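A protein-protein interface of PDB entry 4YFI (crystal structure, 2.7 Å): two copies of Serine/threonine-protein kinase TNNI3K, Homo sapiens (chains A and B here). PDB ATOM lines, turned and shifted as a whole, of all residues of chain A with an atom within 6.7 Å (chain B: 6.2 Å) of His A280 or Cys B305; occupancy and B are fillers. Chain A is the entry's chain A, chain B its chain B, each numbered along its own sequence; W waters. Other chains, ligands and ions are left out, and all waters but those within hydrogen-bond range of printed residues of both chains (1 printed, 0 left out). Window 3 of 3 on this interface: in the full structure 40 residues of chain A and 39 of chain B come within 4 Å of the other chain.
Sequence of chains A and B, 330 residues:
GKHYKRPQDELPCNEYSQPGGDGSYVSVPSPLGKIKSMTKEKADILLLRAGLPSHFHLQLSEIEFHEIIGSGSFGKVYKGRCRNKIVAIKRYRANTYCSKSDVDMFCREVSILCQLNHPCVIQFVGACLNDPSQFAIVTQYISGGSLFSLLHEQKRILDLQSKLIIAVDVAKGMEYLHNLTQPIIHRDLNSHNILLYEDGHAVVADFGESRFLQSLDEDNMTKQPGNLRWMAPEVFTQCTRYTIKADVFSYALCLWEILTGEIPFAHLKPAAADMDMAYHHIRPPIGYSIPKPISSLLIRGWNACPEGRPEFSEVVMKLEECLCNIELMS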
ATOM      1  N   GLU A 234      -8.888 -28.322   9.408  1.00  0.00           N
ATOM      2  CA  GLU A 234      -7.790 -29.292   9.512  1.00  0.00           C
ATOM      3  C   GLU A 234      -7.609 -30.200   8.282  1.00  0.00           C
ATOM      4  O   GLU A 234      -6.720 -31.041   8.268  1.00  0.00           O
ATOM      5  CB  GLU A 234      -7.956 -30.171  10.754  1.00  0.00           C
ATOM      6  CG  GLU A 234      -9.008 -31.273  10.653  1.00  0.00           C
ATOM      7  CD  GLU A 234     -10.394 -30.818  11.081  1.00  0.00           C
ATOM      8  OE1 GLU A 234     -10.658 -29.589  11.166  1.00  0.00           O
ATOM      9  OE2 GLU A 234     -11.226 -31.710  11.335  1.00  0.00           O
ATOM     10  N   ASP A 274       0.702 -28.274  20.742  1.00  0.00           N
ATOM     11  CA  ASP A 274       0.387 -28.243  19.311  1.00  0.00           C
ATOM     12  C   ASP A 274      -1.119 -28.133  19.088  1.00  0.00           C
ATOM     13  O   ASP A 274      -1.593 -27.338  18.283  1.00  0.00           O
ATOM     14  CB  ASP A 274       0.903 -29.503  18.612  1.00  0.00           C
ATOM     15  N   MET A 275      -1.866 -28.947  19.814  1.00  0.00           N
ATOM     16  CA  MET A 275      -3.314 -28.963  19.685  1.00  0.00           C
ATOM     17  C   MET A 275      -3.917 -27.590  20.032  1.00  0.00           C
ATOM     18  O   MET A 275      -4.689 -27.029  19.249  1.00  0.00           O
ATOM     19  CB  MET A 275      -3.897 -30.071  20.573  1.00  0.00           C
ATOM     20  N   ASP A 276      -3.539 -27.031  21.182  1.00  0.00           N
ATOM     21  CA  ASP A 276      -4.070 -25.728  21.592  1.00  0.00           C
ATOM     22  C   ASP A 276      -3.763 -24.647  20.569  1.00  0.00           C
ATOM     23  O   ASP A 276      -4.583 -23.773  20.303  1.00  0.00           O
ATOM     24  CB  ASP A 276      -3.516 -25.319  22.959  1.00  0.00           C
ATOM     25  CG  ASP A 276      -4.061 -26.174  24.089  1.00  0.00           C
ATOM     26  OD1 ASP A 276      -4.793 -27.144  23.809  1.00  0.00           O
ATOM     27  OD2 ASP A 276      -3.758 -25.870  25.258  1.00  0.00           O
ATOM     28  N   MET A 277      -2.569 -24.717  20.002  1.00  0.00           N
ATOM     29  CA  MET A 277      -2.139 -23.747  18.993  1.00  0.00           C
ATOM     30  C   MET A 277      -2.926 -23.885  17.680  1.00  0.00           C
ATOM     31  O   MET A 277      -3.285 -22.881  17.061  1.00  0.00           O
ATOM     32  CB  MET A 277      -0.622 -23.873  18.730  1.00  0.00           C
ATOM     33  CG  MET A 277       0.253 -23.385  19.878  1.00  0.00           C
ATOM     34  SD  MET A 277       1.971 -23.108  19.430  1.00  0.00           S
ATOM     35  CE  MET A 277       2.570 -24.771  19.191  1.00  0.00           C
ATOM     36  N   ALA A 278      -3.202 -25.119  17.266  1.00  0.00           N
ATOM     37  CA  ALA A 278      -3.816 -25.375  15.961  1.00  0.00           C
ATOM     38  C   ALA A 278      -5.344 -25.238  15.995  1.00  0.00           C
ATOM     39  O   ALA A 278      -5.932 -24.476  15.235  1.00  0.00           O
ATOM     40  CB  ALA A 278      -3.417 -26.759  15.462  1.00  0.00           C
ATOM     41  N   TYR A 279      -5.980 -25.968  16.896  1.00  0.00           N
ATOM     42  CA  TYR A 279      -7.433 -26.035  16.933  1.00  0.00           C
ATOM     43  C   TYR A 279      -8.097 -24.897  17.720  1.00  0.00           C
ATOM     44  O   TYR A 279      -9.173 -24.422  17.346  1.00  0.00           O
ATOM     45  CB  TYR A 279      -7.862 -27.363  17.533  1.00  0.00           C
ATOM     46  CG  TYR A 279      -7.270 -28.570  16.855  1.00  0.00           C
ATOM     47  CD1 TYR A 279      -7.246 -28.675  15.470  1.00  0.00           C
ATOM     48  CD2 TYR A 279      -6.767 -29.621  17.605  1.00  0.00           C
ATOM     49  CE1 TYR A 279      -6.721 -29.796  14.857  1.00  0.00           C
ATOM     50  CE2 TYR A 279      -6.237 -30.731  17.000  1.00  0.00           C
ATOM     51  CZ  TYR A 279      -6.221 -30.815  15.628  1.00  0.00           C
ATOM     52  OH  TYR A 279      -5.676 -31.927  15.036  1.00  0.00           O
ATOM     53  N   HIS A 280      -7.476 -24.482  18.819  1.00  0.00           N
ATOM     54  CA  HIS A 280      -8.031 -23.419  19.660  1.00  0.00           C
ATOM     55  C   HIS A 280      -7.427 -22.049  19.363  1.00  0.00           C
ATOM     56  O   HIS A 280      -7.935 -21.051  19.839  1.00  0.00           O
ATOM     57  CB  HIS A 280      -7.872 -23.789  21.139  1.00  0.00           C
ATOM     58  CG  HIS A 280      -8.639 -25.014  21.533  1.00  0.00           C
ATOM     59  ND1 HIS A 280      -9.979 -24.979  21.852  1.00  0.00           N
ATOM     60  CD2 HIS A 280      -8.258 -26.310  21.644  1.00  0.00           C
ATOM     61  CE1 HIS A 280     -10.389 -26.202  22.150  1.00  0.00           C
ATOM     62  NE2 HIS A 280      -9.365 -27.029  22.030  1.00  0.00           N
ATOM     63  N   HIS A 281      -6.356 -22.011  18.567  1.00  0.00           N
ATOM     64  CA  HIS A 281      -5.677 -20.766  18.190  1.00  0.00           C
ATOM     65  C   HIS A 281      -5.062 -20.003  19.377  1.00  0.00           C
ATOM     66  O   HIS A 281      -4.963 -18.777  19.362  1.00  0.00           O
ATOM     67  CB  HIS A 281      -6.613 -19.865  17.376  1.00  0.00           C
ATOM     68  CG  HIS A 281      -6.832 -20.340  15.969  1.00  0.00           C
ATOM     69  ND1 HIS A 281      -6.688 -19.516  14.871  1.00  0.00           N
ATOM     70  CD2 HIS A 281      -7.187 -21.556  15.483  1.00  0.00           C
ATOM     71  CE1 HIS A 281      -6.946 -20.203  13.771  1.00  0.00           C
ATOM     72  NE2 HIS A 281      -7.248 -21.443  14.114  1.00  0.00           N
ATOM     73  N   ILE A 282      -4.604 -20.744  20.382  1.00  0.00           N
ATOM     74  CA  ILE A 282      -3.970 -20.156  21.560  1.00  0.00           C
ATOM     75  C   ILE A 282      -2.467 -19.952  21.326  1.00  0.00           C
ATOM     76  O   ILE A 282      -1.832 -20.754  20.642  1.00  0.00           O
ATOM     77  CB  ILE A 282      -4.226 -21.046  22.799  1.00  0.00           C
ATOM     78  CG1 ILE A 282      -5.719 -21.000  23.154  1.00  0.00           C
ATOM     79  CG2 ILE A 282      -3.401 -20.604  24.002  1.00  0.00           C
ATOM     80  CD1 ILE A 282      -6.211 -22.255  23.838  1.00  0.00           C
ATOM     81  N   ARG A 283      -1.925 -18.865  21.881  1.00  0.00           N
ATOM     82  CA  ARG A 283      -0.493 -18.566  21.819  1.00  0.00           C
ATOM     83  C   ARG A 283       0.045 -18.294  23.212  1.00  0.00           C
ATOM     84  O   ARG A 283      -0.698 -17.913  24.095  1.00  0.00           O
ATOM     85  CB  ARG A 283      -0.219 -17.332  20.956  1.00  0.00           C
ATOM     86  CG  ARG A 283      -0.647 -17.460  19.504  1.00  0.00           C
ATOM     87  CD  ARG A 283       0.131 -18.525  18.736  1.00  0.00           C
ATOM     88  NE  ARG A 283      -0.375 -18.644  17.363  1.00  0.00           N
ATOM     89  CZ  ARG A 283      -1.174 -19.612  16.903  1.00  0.00           C
ATOM     90  NH1 ARG A 283      -1.545 -19.588  15.639  1.00  0.00           N
ATOM     91  NH2 ARG A 283      -1.584 -20.616  17.678  1.00  0.00           N
ATOM     92  N   HIS B 281     -11.124 -17.581  11.420  1.00  0.00           N
ATOM     93  CA  HIS B 281     -12.308 -18.048  12.160  1.00  0.00           C
ATOM     94  C   HIS B 281     -13.676 -17.638  11.657  1.00  0.00           C
ATOM     95  O   HIS B 281     -14.667 -17.827  12.365  1.00  0.00           O
ATOM     96  CB  HIS B 281     -12.245 -17.572  13.598  1.00  0.00           C
ATOM     97  CG  HIS B 281     -11.157 -18.199  14.394  1.00  0.00           C
ATOM     98  ND1 HIS B 281     -11.009 -19.564  14.502  1.00  0.00           N
ATOM     99  CD2 HIS B 281     -10.187 -17.646  15.159  1.00  0.00           C
ATOM    100  CE1 HIS B 281      -9.981 -19.828  15.286  1.00  0.00           C
ATOM    101  NE2 HIS B 281      -9.466 -18.680  15.698  1.00  0.00           N
ATOM    102  N   ARG B 300     -21.583 -25.707  17.254  1.00  0.00           N
ATOM    103  CA  ARG B 300     -20.741 -26.827  17.697  1.00  0.00           C
ATOM    104  C   ARG B 300     -20.193 -27.646  16.503  1.00  0.00           C
ATOM    105  O   ARG B 300     -19.012 -28.045  16.493  1.00  0.00           O
ATOM    106  CB  ARG B 300     -21.521 -27.726  18.652  1.00  0.00           C
ATOM    107  CG  ARG B 300     -21.773 -27.104  20.019  1.00  0.00           C
ATOM    108  CD  ARG B 300     -22.954 -27.780  20.706  1.00  0.00           C
ATOM    109  NE  ARG B 300     -22.691 -29.202  20.882  1.00  0.00           N
ATOM    110  CZ  ARG B 300     -23.607 -30.169  20.872  1.00  0.00           C
ATOM    111  NH1 ARG B 300     -24.900 -29.901  20.681  1.00  0.00           N
ATOM    112  NH2 ARG B 300     -23.220 -31.428  21.046  1.00  0.00           N
ATOM    113  N   TRP B 302     -19.385 -26.612  13.499  1.00  0.00           N
ATOM    114  CA  TRP B 302     -18.209 -25.996  12.851  1.00  0.00           C
ATOM    115  C   TRP B 302     -17.194 -25.389  13.826  1.00  0.00           C
ATOM    116  O   TRP B 302     -16.389 -24.541  13.447  1.00  0.00           O
ATOM    117  CB  TRP B 302     -18.590 -25.003  11.735  1.00  0.00           C
ATOM    118  CG  TRP B 302     -19.489 -23.875  12.093  1.00  0.00           C
ATOM    119  CD1 TRP B 302     -19.413 -23.064  13.188  1.00  0.00           C
ATOM    120  CD2 TRP B 302     -20.572 -23.379  11.302  1.00  0.00           C
ATOM    121  NE1 TRP B 302     -20.407 -22.122  13.146  1.00  0.00           N
ATOM    122  CE2 TRP B 302     -21.126 -22.283  11.994  1.00  0.00           C
ATOM    123  CE3 TRP B 302     -21.128 -23.755  10.077  1.00  0.00           C
ATOM    124  CZ2 TRP B 302     -22.220 -21.568  11.511  1.00  0.00           C
ATOM    125  CZ3 TRP B 302     -22.218 -23.050   9.598  1.00  0.00           C
ATOM    126  CH2 TRP B 302     -22.750 -21.963  10.314  1.00  0.00           C
ATOM    127  N   ASN B 303     -17.203 -25.876  15.063  1.00  0.00           N
ATOM    128  CA  ASN B 303     -16.138 -25.577  16.015  1.00  0.00           C
ATOM    129  C   ASN B 303     -14.786 -25.874  15.376  1.00  0.00           C
ATOM    130  O   ASN B 303     -14.639 -26.858  14.677  1.00  0.00           O
ATOM    131  CB  ASN B 303     -16.327 -26.405  17.305  1.00  0.00           C
ATOM    132  CG  ASN B 303     -15.425 -25.958  18.464  1.00  0.00           C
ATOM    133  OD1 ASN B 303     -14.223 -25.698  18.314  1.00  0.00           O
ATOM    134  ND2 ASN B 303     -16.007 -25.919  19.641  1.00  0.00           N
ATOM    135  N   ALA B 304     -13.814 -25.000  15.610  1.00  0.00           N
ATOM    136  CA  ALA B 304     -12.468 -25.185  15.076  1.00  0.00           C
ATOM    137  C   ALA B 304     -11.750 -26.402  15.668  1.00  0.00           C
ATOM    138  O   ALA B 304     -10.862 -26.972  15.027  1.00  0.00           O
ATOM    139  CB  ALA B 304     -11.651 -23.927  15.290  1.00  0.00           C
ATOM    140  N   CYS B 305     -12.124 -26.781  16.894  1.00  0.00           N
ATOM    141  CA  CYS B 305     -11.635 -28.015  17.514  1.00  0.00           C
ATOM    142  C   CYS B 305     -12.531 -29.177  17.088  1.00  0.00           C
ATOM    143  O   CYS B 305     -13.711 -29.174  17.395  1.00  0.00           O
ATOM    144  CB  CYS B 305     -11.633 -27.885  19.038  1.00  0.00           C
ATOM    145  SG  CYS B 305     -10.850 -29.270  19.912  1.00  0.00           S
ATOM    146  N   PRO B 306     -11.988 -30.156  16.348  1.00  0.00           N
ATOM    147  CA  PRO B 306     -12.760 -31.343  16.001  1.00  0.00           C
ATOM    148  C   PRO B 306     -13.492 -31.995  17.187  1.00  0.00           C
ATOM    149  O   PRO B 306     -14.676 -32.272  17.086  1.00  0.00           O
ATOM    150  CB  PRO B 306     -11.696 -32.290  15.445  1.00  0.00           C
ATOM    151  CG  PRO B 306     -10.691 -31.388  14.832  1.00  0.00           C
ATOM    152  CD  PRO B 306     -10.696 -30.121  15.638  1.00  0.00           C
ATOM    153  N   GLU B 307     -12.800 -32.207  18.300  1.00  0.00           N
ATOM    154  CA  GLU B 307     -13.368 -32.902  19.476  1.00  0.00           C
ATOM    155  C   GLU B 307     -14.600 -32.192  20.073  1.00  0.00           C
ATOM    156  O   GLU B 307     -15.419 -32.812  20.742  1.00  0.00           O
ATOM    157  CB  GLU B 307     -12.304 -33.091  20.577  1.00  0.00           C
ATOM    158  CG  GLU B 307     -11.102 -33.960  20.189  1.00  0.00           C
ATOM    159  CD  GLU B 307      -9.999 -33.203  19.429  1.00  0.00           C
ATOM    160  OE1 GLU B 307      -9.597 -32.090  19.857  1.00  0.00           O
ATOM    161  OE2 GLU B 307      -9.523 -33.722  18.390  1.00  0.00           O
ATOM    162  N   GLY B 308     -14.713 -30.892  19.837  1.00  0.00           N
ATOM    163  CA  GLY B 308     -15.897 -30.132  20.214  1.00  0.00           C
ATOM    164  C   GLY B 308     -17.096 -30.390  19.324  1.00  0.00           C
ATOM    165  O   GLY B 308     -18.231 -30.100  19.707  1.00  0.00           O
ATOM    166  N   ARG B 309     -16.857 -30.919  18.129  1.00  0.00           N
ATOM    167  CA  ARG B 309     -17.938 -31.193  17.198  1.00  0.00           C
ATOM    168  C   ARG B 309     -18.759 -32.398  17.632  1.00  0.00           C
ATOM    169  O   ARG B 309     -18.207 -33.384  18.101  1.00  0.00           O
ATOM    170  CB  ARG B 309     -17.403 -31.421  15.782  1.00  0.00           C
ATOM    171  CG  ARG B 309     -16.813 -30.178  15.157  1.00  0.00           C
ATOM    172  CD  ARG B 309     -16.118 -30.477  13.849  1.00  0.00           C
ATOM    173  NE  ARG B 309     -15.078 -29.488  13.607  1.00  0.00           N
ATOM    174  CZ  ARG B 309     -14.008 -29.672  12.842  1.00  0.00           C
ATOM    175  NH1 ARG B 309     -13.810 -30.816  12.188  1.00  0.00           N
ATOM    176  NH2 ARG B 309     -13.127 -28.691  12.722  1.00  0.00           N
HETATM  177  O   HOH W   1     -11.042 -28.969  22.819  1.00  0.00           O
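OE2 of Glu A234 lies within salt-bridge range of NH1 of Arg B309, at 2.9 Å. A ring nitrogen (NE2) of His A280 sits at hydrogen-bond distance from the side-chain sulfur (SG) of Cys B305, 3.4 Å away. A ring nitrogen (ND1) of His A281 is in hydrogen-bond range of a ring nitrogen (NE2) of His B281 (3.0 Å).
N of Cys B305 is in hydrogen-bond range of OD1 of Asn B303, 2.8 Å away. The backbone carbonyl oxygen (O) of Ala A278 lies close to a ring nitrogen (NE2) of His A281, 3.5 Å away. The guanidinium group of Arg B309 is in hydrogen-bond range of the backbone carbonyl oxygen of Asn B303 (2.9 Å). OE1 of Glu B307 is in hydrogen-bond range of SG of Cys B305, at 3.1 Å. The backbone carbonyl oxygen (O) of Asp A276 lies within hydrogen-bond range of the backbone NH (N) of His A281, at 3.0 Å.
Among the printed residues, merely in contact across the chains: Tyr A279 with Ala B304, Glu A234 with Pro B306, Tyr A279 with Pro B306 and Tyr A279 with Cys B305.
Printed residues of chain B within 4 Å of Glu A234: Pro B306 (3.6 Å) and Arg B309 (2.9 Å). Arg A283 touches none of the printed residues of chain B. Of the printed residues of chain A, His B281 touches His A281. Trp B302 touches none of the printed residues of chain A. Of chain A, only Tyr A279 (3.8 Å) and His A280 (3.4 Å) come within 4 Å of Cys B305. Printed residues of chain A within 4 Å of Pro B306: Glu A234 and Tyr A279. The nearest residue of chain B that does not touch His A280 is His B281 (5.0 Å). The nearest residue of chain A that does not touch Cys B305 is Glu A234 (6.2 Å).
Hydrophobic or aromatic side chains of chain A within 4 Å of the printed part of chain B: Tyr A279, His A280 and His A281. Among the printed residues, Asp or Glu carboxylates within 4 Å of a Lys or Arg side-chain nitrogen of the other chain: Glu A234 with Arg B309.
His A281 touches its own counterpart, His B281. Position printed for both chains: 281. Of the 7 pairs that touch across the chains among the printed residues, 1 has its exchanged pair printed and touching as well.
Water W1 lies within hydrogen-bond range of NE2 of His A280 (2.7 Å) and SG of Cys B305 (2.9 Å).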
